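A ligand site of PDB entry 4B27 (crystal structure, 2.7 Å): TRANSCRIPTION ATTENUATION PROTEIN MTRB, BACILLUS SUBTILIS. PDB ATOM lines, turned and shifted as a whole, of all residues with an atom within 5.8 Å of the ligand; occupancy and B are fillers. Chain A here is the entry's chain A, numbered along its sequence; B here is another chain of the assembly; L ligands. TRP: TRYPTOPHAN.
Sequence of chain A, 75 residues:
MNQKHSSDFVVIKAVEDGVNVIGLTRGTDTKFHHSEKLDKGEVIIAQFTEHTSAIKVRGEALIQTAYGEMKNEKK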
ATOM      1  N   LEU A  24     -14.248 -22.279 -21.992  1.00  0.00           N
ATOM      2  CA  LEU A  24     -14.496 -20.950 -21.410  1.00  0.00           C
ATOM      3  C   LEU A  24     -15.937 -20.515 -21.665  1.00  0.00           C
ATOM      4  O   LEU A  24     -16.417 -20.594 -22.791  1.00  0.00           O
ATOM      5  CB  LEU A  24     -13.547 -19.901 -21.983  1.00  0.00           C
ATOM      6  CG  LEU A  24     -12.081 -19.873 -21.513  1.00  0.00           C
ATOM      7  CD1 LEU A  24     -11.274 -21.050 -22.059  1.00  0.00           C
ATOM      8  CD2 LEU A  24     -11.456 -18.577 -21.985  1.00  0.00           C
ATOM      9  N   THR A  25     -16.607 -20.059 -20.608  1.00  0.00           N
ATOM     10  CA  THR A  25     -18.050 -19.738 -20.622  1.00  0.00           C
ATOM     11  C   THR A  25     -18.394 -18.680 -21.667  1.00  0.00           C
ATOM     12  O   THR A  25     -17.678 -17.691 -21.806  1.00  0.00           O
ATOM     13  CB  THR A  25     -18.586 -19.230 -19.246  1.00  0.00           C
ATOM     14  OG1 THR A  25     -17.991 -17.964 -18.899  1.00  0.00           O
ATOM     15  CG2 THR A  25     -18.301 -20.204 -18.138  1.00  0.00           C
ATOM     16  N   ARG A  26     -19.468 -18.913 -22.408  1.00  0.00           N
ATOM     17  CA  ARG A  26     -20.058 -17.895 -23.284  1.00  0.00           C
ATOM     18  C   ARG A  26     -20.987 -17.018 -22.451  1.00  0.00           C
ATOM     19  O   ARG A  26     -21.729 -17.532 -21.608  1.00  0.00           O
ATOM     20  CB  ARG A  26     -20.823 -18.538 -24.448  1.00  0.00           C
ATOM     21  CG  ARG A  26     -21.827 -17.642 -25.160  1.00  0.00           C
ATOM     22  CD  ARG A  26     -22.801 -18.411 -26.046  1.00  0.00           C
ATOM     23  NE  ARG A  26     -22.129 -19.467 -26.806  1.00  0.00           N
ATOM     24  CZ  ARG A  26     -21.430 -19.261 -27.928  1.00  0.00           C
ATOM     25  NH1 ARG A  26     -21.313 -18.036 -28.448  1.00  0.00           N
ATOM     26  NH2 ARG A  26     -20.847 -20.289 -28.525  1.00  0.00           N
ATOM     27  N   GLY A  27     -20.943 -15.702 -22.665  1.00  0.00           N
ATOM     28  CA  GLY A  27     -21.817 -14.807 -21.932  1.00  0.00           C
ATOM     29  C   GLY A  27     -21.088 -13.514 -21.695  1.00  0.00           C
ATOM     30  O   GLY A  27     -20.037 -13.290 -22.329  1.00  0.00           O
ATOM     31  N   THR A  28     -21.635 -12.667 -20.821  1.00  0.00           N
ATOM     32  CA  THR A  28     -20.961 -11.421 -20.470  1.00  0.00           C
ATOM     33  C   THR A  28     -19.670 -11.806 -19.751  1.00  0.00           C
ATOM     34  O   THR A  28     -18.608 -11.217 -20.001  1.00  0.00           O
ATOM     35  CB  THR A  28     -21.847 -10.467 -19.620  1.00  0.00           C
ATOM     36  OG1 THR A  28     -22.056 -11.016 -18.318  1.00  0.00           O
ATOM     37  CG2 THR A  28     -23.216 -10.198 -20.252  1.00  0.00           C
ATOM     38  N   ASP A  29     -19.756 -12.829 -18.898  1.00  0.00           N
ATOM     39  CA  ASP A  29     -18.619 -13.333 -18.124  1.00  0.00           C
ATOM     40  C   ASP A  29     -17.798 -14.340 -18.895  1.00  0.00           C
ATOM     41  O   ASP A  29     -18.312 -15.055 -19.725  1.00  0.00           O
ATOM     42  CB  ASP A  29     -19.128 -14.012 -16.850  1.00  0.00           C
ATOM     43  CG  ASP A  29     -19.693 -13.031 -15.865  1.00  0.00           C
ATOM     44  OD1 ASP A  29     -19.544 -11.790 -16.021  1.00  0.00           O
ATOM     45  OD2 ASP A  29     -20.302 -13.529 -14.899  1.00  0.00           O
ATOM     46  N   THR A  30     -16.516 -14.397 -18.583  1.00  0.00           N
ATOM     47  CA  THR A  30     -15.607 -15.334 -19.234  1.00  0.00           C
ATOM     48  C   THR A  30     -14.774 -16.041 -18.186  1.00  0.00           C
ATOM     49  O   THR A  30     -13.861 -15.432 -17.621  1.00  0.00           O
ATOM     50  CB  THR A  30     -14.655 -14.600 -20.169  1.00  0.00           C
ATOM     51  OG1 THR A  30     -15.381 -13.646 -20.961  1.00  0.00           O
ATOM     52  CG2 THR A  30     -13.940 -15.586 -21.074  1.00  0.00           C
ATOM     53  N   LYS A  31     -15.090 -17.301 -17.917  1.00  0.00           N
ATOM     54  CA  LYS A  31     -14.305 -18.118 -16.982  1.00  0.00           C
ATOM     55  C   LYS A  31     -14.248 -19.580 -17.377  1.00  0.00           C
ATOM     56  O   LYS A  31     -15.010 -20.027 -18.193  1.00  0.00           O
ATOM     57  CB  LYS A  31     -14.793 -17.947 -15.526  1.00  0.00           C
ATOM     58  CG  LYS A  31     -16.290 -17.887 -15.319  1.00  0.00           C
ATOM     59  CD  LYS A  31     -16.565 -17.106 -14.034  1.00  0.00           C
ATOM     60  CE  LYS A  31     -17.849 -17.539 -13.334  1.00  0.00           C
ATOM     61  NZ  LYS A  31     -17.944 -16.853 -12.018  1.00  0.00           N
ATOM     62  N   SER A  53     -17.681 -20.784 -25.731  1.00  0.00           N
ATOM     63  CA  SER A  53     -17.400 -19.918 -26.872  1.00  0.00           C
ATOM     64  C   SER A  53     -15.899 -19.770 -27.152  1.00  0.00           C
ATOM     65  O   SER A  53     -15.486 -19.127 -28.119  1.00  0.00           O
ATOM     66  CB  SER A  53     -18.091 -18.559 -26.671  1.00  0.00           C
ATOM     67  OG  SER A  53     -17.550 -17.861 -25.574  1.00  0.00           O
ATOM     68  N   ALA A  54     -15.094 -20.376 -26.288  1.00  0.00           N
ATOM     69  CA  ALA A  54     -13.660 -20.405 -26.475  1.00  0.00           C
ATOM     70  C   ALA A  54     -13.035 -21.577 -25.754  1.00  0.00           C
ATOM     71  O   ALA A  54     -13.434 -21.947 -24.647  1.00  0.00           O
ATOM     72  CB  ALA A  54     -13.042 -19.097 -26.023  1.00  0.00           C
ATOM     73  N   VAL B  21      -4.504 -12.038 -24.918  1.00  0.00           N
ATOM     74  CA  VAL B  21      -5.635 -12.046 -25.849  1.00  0.00           C
ATOM     75  C   VAL B  21      -6.829 -11.332 -25.260  1.00  0.00           C
ATOM     76  O   VAL B  21      -7.319 -11.687 -24.175  1.00  0.00           O
ATOM     77  CB  VAL B  21      -6.022 -13.476 -26.251  1.00  0.00           C
ATOM     78  CG1 VAL B  21      -7.330 -13.484 -27.014  1.00  0.00           C
ATOM     79  CG2 VAL B  21      -4.915 -14.128 -27.086  1.00  0.00           C
ATOM     80  N   ILE B  22      -7.296 -10.323 -25.976  1.00  0.00           N
ATOM     81  CA  ILE B  22      -8.281  -9.401 -25.432  1.00  0.00           C
ATOM     82  C   ILE B  22      -9.581  -9.374 -26.220  1.00  0.00           C
ATOM     83  O   ILE B  22      -9.591  -9.094 -27.421  1.00  0.00           O
ATOM     84  CB  ILE B  22      -7.717  -7.971 -25.367  1.00  0.00           C
ATOM     85  CG1 ILE B  22      -6.357  -7.951 -24.663  1.00  0.00           C
ATOM     86  CG2 ILE B  22      -8.680  -7.047 -24.640  1.00  0.00           C
ATOM     87  CD1 ILE B  22      -5.180  -7.939 -25.618  1.00  0.00           C
ATOM     88  N   GLY B  23     -10.672  -9.682 -25.532  1.00  0.00           N
ATOM     89  CA  GLY B  23     -11.997  -9.576 -26.131  1.00  0.00           C
ATOM     90  C   GLY B  23     -12.506  -8.175 -25.942  1.00  0.00           C
ATOM     91  O   GLY B  23     -12.398  -7.638 -24.845  1.00  0.00           O
ATOM     92  N   LEU B  24     -13.050  -7.593 -27.004  1.00  0.00           N
ATOM     93  CA  LEU B  24     -13.616  -6.229 -26.981  1.00  0.00           C
ATOM     94  C   LEU B  24     -15.115  -6.280 -27.162  1.00  0.00           C
ATOM     95  O   LEU B  24     -15.597  -6.949 -28.086  1.00  0.00           O
ATOM     96  CB  LEU B  24     -13.021  -5.383 -28.100  1.00  0.00           C
ATOM     97  CG  LEU B  24     -11.596  -4.827 -27.985  1.00  0.00           C
ATOM     98  CD1 LEU B  24     -10.526  -5.921 -28.084  1.00  0.00           C
ATOM     99  CD2 LEU B  24     -11.422  -3.801 -29.102  1.00  0.00           C
ATOM    100  N   HIS B  33     -13.274  -6.494 -22.041  1.00  0.00           N
ATOM    101  CA  HIS B  33     -14.118  -7.143 -21.019  1.00  0.00           C
ATOM    102  C   HIS B  33     -13.439  -8.372 -20.469  1.00  0.00           C
ATOM    103  O   HIS B  33     -13.761  -8.850 -19.382  1.00  0.00           O
ATOM    104  CB  HIS B  33     -15.491  -7.496 -21.562  1.00  0.00           C
ATOM    105  CG  HIS B  33     -15.474  -8.581 -22.609  1.00  0.00           C
ATOM    106  ND1 HIS B  33     -15.700  -9.877 -22.311  1.00  0.00           N
ATOM    107  CD2 HIS B  33     -15.219  -8.529 -23.982  1.00  0.00           C
ATOM    108  CE1 HIS B  33     -15.599 -10.615 -23.442  1.00  0.00           C
ATOM    109  NE2 HIS B  33     -15.304  -9.783 -24.458  1.00  0.00           N
ATOM    110  N   HIS B  34     -12.502  -8.913 -21.242  1.00  0.00           N
ATOM    111  CA  HIS B  34     -11.673 -10.017 -20.802  1.00  0.00           C
ATOM    112  C   HIS B  34     -10.324 -10.022 -21.464  1.00  0.00           C
ATOM    113  O   HIS B  34     -10.178  -9.767 -22.671  1.00  0.00           O
ATOM    114  CB  HIS B  34     -12.379 -11.338 -21.046  1.00  0.00           C
ATOM    115  CG  HIS B  34     -11.566 -12.540 -20.606  1.00  0.00           C
ATOM    116  ND1 HIS B  34     -11.683 -13.079 -19.377  1.00  0.00           N
ATOM    117  CD2 HIS B  34     -10.605 -13.294 -21.275  1.00  0.00           C
ATOM    118  CE1 HIS B  34     -10.842 -14.128 -19.276  1.00  0.00           C
ATOM    119  NE2 HIS B  34     -10.184 -14.256 -20.433  1.00  0.00           N
ATOM    120  N   SER B  35      -9.323 -10.344 -20.664  1.00  0.00           N
ATOM    121  CA  SER B  35      -7.974 -10.525 -21.157  1.00  0.00           C
ATOM    122  C   SER B  35      -7.455 -11.893 -20.696  1.00  0.00           C
ATOM    123  O   SER B  35      -7.241 -12.116 -19.495  1.00  0.00           O
ATOM    124  CB  SER B  35      -7.106  -9.393 -20.616  1.00  0.00           C
ATOM    125  OG  SER B  35      -5.747  -9.584 -20.939  1.00  0.00           O
ATOM    126  N   GLU B  36      -7.300 -12.819 -21.640  1.00  0.00           N
ATOM    127  CA  GLU B  36      -6.760 -14.147 -21.307  1.00  0.00           C
ATOM    128  C   GLU B  36      -5.275 -14.237 -21.624  1.00  0.00           C
ATOM    129  O   GLU B  36      -4.849 -13.955 -22.746  1.00  0.00           O
ATOM    130  CB  GLU B  36      -7.554 -15.253 -22.024  1.00  0.00           C
ATOM    131  CG  GLU B  36      -7.205 -16.689 -21.598  1.00  0.00           C
ATOM    132  CD  GLU B  36      -7.769 -17.072 -20.234  1.00  0.00           C
ATOM    133  OE1 GLU B  36      -8.845 -16.557 -19.840  1.00  0.00           O
ATOM    134  OE2 GLU B  36      -7.147 -17.917 -19.553  1.00  0.00           O
ATOM    135  N   ALA B  46     -10.803 -18.981 -30.232  1.00  0.00           N
ATOM    136  CA  ALA B  46     -11.854 -18.104 -29.785  1.00  0.00           C
ATOM    137  C   ALA B  46     -12.806 -17.756 -30.908  1.00  0.00           C
ATOM    138  O   ALA B  46     -12.391 -17.390 -32.007  1.00  0.00           O
ATOM    139  CB  ALA B  46     -11.272 -16.853 -29.158  1.00  0.00           C
ATOM    140  N   GLN B  47     -14.081 -17.880 -30.595  1.00  0.00           N
ATOM    141  CA  GLN B  47     -15.164 -17.481 -31.474  1.00  0.00           C
ATOM    142  C   GLN B  47     -15.431 -16.010 -31.247  1.00  0.00           C
ATOM    143  O   GLN B  47     -15.111 -15.484 -30.185  1.00  0.00           O
ATOM    144  CB  GLN B  47     -16.434 -18.215 -31.060  1.00  0.00           C
ATOM    145  CG  GLN B  47     -16.482 -19.691 -31.383  1.00  0.00           C
ATOM    146  CD  GLN B  47     -17.923 -20.173 -31.563  1.00  0.00           C
ATOM    147  OE1 GLN B  47     -18.833 -19.708 -30.852  1.00  0.00           O
ATOM    148  NE2 GLN B  47     -18.135 -21.073 -32.542  1.00  0.00           N
ATOM    149  N   PHE B  48     -16.001 -15.353 -32.264  1.00  0.00           N
ATOM    150  CA  PHE B  48     -16.705 -14.093 -32.080  1.00  0.00           C
ATOM    151  C   PHE B  48     -18.093 -14.459 -31.617  1.00  0.00           C
ATOM    152  O   PHE B  48     -18.620 -15.488 -32.003  1.00  0.00           O
ATOM    153  CB  PHE B  48     -16.787 -13.303 -33.388  1.00  0.00           C
ATOM    154  CG  PHE B  48     -15.482 -12.665 -33.797  1.00  0.00           C
ATOM    155  CD1 PHE B  48     -15.035 -11.504 -33.179  1.00  0.00           C
ATOM    156  CD2 PHE B  48     -14.699 -13.242 -34.805  1.00  0.00           C
ATOM    157  CE1 PHE B  48     -13.839 -10.933 -33.559  1.00  0.00           C
ATOM    158  CE2 PHE B  48     -13.495 -12.673 -35.190  1.00  0.00           C
ATOM    159  CZ  PHE B  48     -13.070 -11.514 -34.568  1.00  0.00           C
ATOM    160  N   THR B  49     -18.665 -13.615 -30.786  1.00  0.00           N
ATOM    161  CA  THR B  49     -19.833 -13.993 -29.991  1.00  0.00           C
ATOM    162  C   THR B  49     -20.741 -12.827 -29.787  1.00  0.00           C
ATOM    163  O   THR B  49     -20.441 -11.701 -30.205  1.00  0.00           O
ATOM    164  CB  THR B  49     -19.372 -14.386 -28.584  1.00  0.00           C
ATOM    165  OG1 THR B  49     -19.042 -13.184 -27.859  1.00  0.00           O
ATOM    166  CG2 THR B  49     -18.139 -15.286 -28.657  1.00  0.00           C
ATOM    167  N   GLU B  50     -21.839 -13.066 -29.082  1.00  0.00           N
ATOM    168  CA  GLU B  50     -22.785 -11.996 -28.793  1.00  0.00           C
ATOM    169  C   GLU B  50     -22.107 -10.846 -28.075  1.00  0.00           C
ATOM    170  O   GLU B  50     -22.557  -9.692 -28.183  1.00  0.00           O
ATOM    171  CB  GLU B  50     -23.953 -12.535 -27.981  1.00  0.00           C
ATOM    172  CG  GLU B  50     -25.054 -11.520 -27.688  1.00  0.00           C
ATOM    173  CD  GLU B  50     -26.137 -12.091 -26.795  1.00  0.00           C
ATOM    174  OE1 GLU B  50     -26.102 -13.322 -26.504  1.00  0.00           O
ATOM    175  OE2 GLU B  50     -27.027 -11.329 -26.381  1.00  0.00           O
ATOM    176  N   HIS B  51     -21.020 -11.135 -27.366  1.00  0.00           N
ATOM    177  CA  HIS B  51     -20.311 -10.113 -26.571  1.00  0.00           C
ATOM    178  C   HIS B  51     -18.956  -9.697 -27.076  1.00  0.00           C
ATOM    179  O   HIS B  51     -18.435  -8.681 -26.673  1.00  0.00           O
ATOM    180  CB  HIS B  51     -20.239 -10.552 -25.120  1.00  0.00           C
ATOM    181  CG  HIS B  51     -21.605 -10.757 -24.509  1.00  0.00           C
ATOM    182  ND1 HIS B  51     -22.246 -11.947 -24.558  1.00  0.00           N
ATOM    183  CD2 HIS B  51     -22.468  -9.869 -23.879  1.00  0.00           C
ATOM    184  CE1 HIS B  51     -23.456 -11.819 -23.959  1.00  0.00           C
ATOM    185  NE2 HIS B  51     -23.585 -10.549 -23.535  1.00  0.00           N
ATOM    186  N   THR B  52     -18.388 -10.478 -27.988  1.00  0.00           N
ATOM    187  CA  THR B  52     -17.076 -10.162 -28.519  1.00  0.00           C
ATOM    188  C   THR B  52     -17.134  -9.962 -30.017  1.00  0.00           C
ATOM    189  O   THR B  52     -17.373 -10.912 -30.768  1.00  0.00           O
ATOM    190  CB  THR B  52     -16.083 -11.275 -28.160  1.00  0.00           C
ATOM    191  OG1 THR B  52     -16.011 -11.379 -26.726  1.00  0.00           O
ATOM    192  CG2 THR B  52     -14.692 -10.988 -28.745  1.00  0.00           C
ATOM    193  N   ILE B  55     -11.232  -9.006 -31.396  1.00  0.00           N
ATOM    194  CA  ILE B  55     -10.225  -9.614 -30.570  1.00  0.00           C
ATOM    195  C   ILE B  55      -8.907  -8.924 -30.876  1.00  0.00           C
ATOM    196  O   ILE B  55      -8.581  -8.691 -32.045  1.00  0.00           O
ATOM    197  CB  ILE B  55     -10.101 -11.091 -30.921  1.00  0.00           C
ATOM    198  CG1 ILE B  55     -11.336 -11.838 -30.439  1.00  0.00           C
ATOM    199  CG2 ILE B  55      -8.870 -11.682 -30.270  1.00  0.00           C
ATOM    200  CD1 ILE B  55     -11.501 -13.183 -31.138  1.00  0.00           C
HETATM  201  N   TRP L   1     -17.650 -14.979 -22.419  1.00  0.00           N
HETATM  202  CA  TRP L   1     -16.966 -14.569 -23.627  1.00  0.00           C
HETATM  203  C   TRP L   1     -17.911 -14.590 -24.789  1.00  0.00           C
HETATM  204  O   TRP L   1     -18.829 -15.410 -24.839  1.00  0.00           O
HETATM  205  CB  TRP L   1     -15.796 -15.498 -23.902  1.00  0.00           C
HETATM  206  CG  TRP L   1     -15.043 -15.202 -25.182  1.00  0.00           C
HETATM  207  CD1 TRP L   1     -15.358 -15.658 -26.458  1.00  0.00           C
HETATM  208  CD2 TRP L   1     -13.828 -14.401 -25.350  1.00  0.00           C
HETATM  209  NE1 TRP L   1     -14.457 -15.188 -27.374  1.00  0.00           N
HETATM  210  CE2 TRP L   1     -13.512 -14.439 -26.781  1.00  0.00           C
HETATM  211  CE3 TRP L   1     -13.002 -13.676 -24.494  1.00  0.00           C
HETATM  212  CZ2 TRP L   1     -12.403 -13.779 -27.316  1.00  0.00           C
HETATM  213  CZ3 TRP L   1     -11.899 -13.015 -25.041  1.00  0.00           C
HETATM  214  CH2 TRP L   1     -11.604 -13.075 -26.415  1.00  0.00           C
HETATM  215  OXT TRP L   1     -17.787 -13.755 -25.711  1.00  0.00           O
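OXT of the ligand is in hydrogen-bond range of OG1 of Thr 49 of chain B (2.6 Å). The backbone carbonyl oxygen (O) of Gly 27 is in hydrogen-bond range of a nitrogen (N) of the ligand. The backbone carbonyl oxygen (O) of Gln 47 of chain B is in hydrogen-bond range of a nitrogen (NE1) of the ligand, 2.9 Å away. The side-chain hydroxyl of Thr 52 of chain B lies within hydrogen-bond range of an oxygen (OXT) of the ligand (3.1 Å). O of Asp 29 is in hydrogen-bond range of N of the ligand (2.8 Å). O of Thr 25 is in hydrogen-bond range of N of the ligand, at 2.8 Å. The side-chain hydroxyl (OG) of Ser 53 is in hydrogen-bond range of an oxygen (O) of the ligand, at 2.9 Å. The side-chain hydroxyl of Thr 30 lies within hydrogen-bond range of a nitrogen (N) of the ligand, 3.0 Å away. The backbone NH (N) of Gly 27 sits at hydrogen-bond distance from an oxygen (O) of the ligand (3.0 Å).
The side-chain carboxylate of Asp 29 is in hydrogen-bond range of the side-chain hydroxyl of Thr 28 (3.5 Å). The backbone carbonyl oxygen (O) of Lys 31 lies within hydrogen-bond range of the backbone NH (N) of Thr 25 (2.9 Å). A ring nitrogen (NE2) of His 33 of chain B is in hydrogen-bond range of the side-chain hydroxyl (OG1) of Thr 52 of chain B, at 2.9 Å. N of Gly 23 of chain B lies within hydrogen-bond range of O of His 34 of chain B, at 2.9 Å. The backbone NH (N) of His 33 of chain B sits close to the backbone carbonyl oxygen (O) of Gly 23 of chain B (3.2 Å). The backbone carbonyl oxygen of Gly 27 lies within hydrogen-bond range of a ring nitrogen (ND1) of His 51 of chain B. NE2 of His 34 of chain B is in hydrogen-bond range of OE1 of Glu 36 of chain B, 2.7 Å away. The backbone carbonyl oxygen (O) of Asp 29 lies within hydrogen-bond range of the side-chain hydroxyl (OG1) of Thr 25 (3.0 Å).
Arg 26 touches the ligand. Gly 23 of chain B touches the ligand (CA to CH2, 3.5 Å). His 34 of chain B touches the ligand. CB of Ala 46 of chain B touches CZ2 of the ligand, at 3.8 Å. Ile 55 of chain B touches the ligand (CG1 to CZ2, 3.8 Å). 13 residues have an atom within 4 Å of the ligand: Thr 25, Arg 26, Gly 27, Asp 29, Thr 30, Ser 53, Gly 23 of chain B, His 34 of chain B, Ala 46 of chain B, Gln 47 of chain B, Thr 49 of chain B, Thr 52 of chain B and Ile 55 of chain B.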
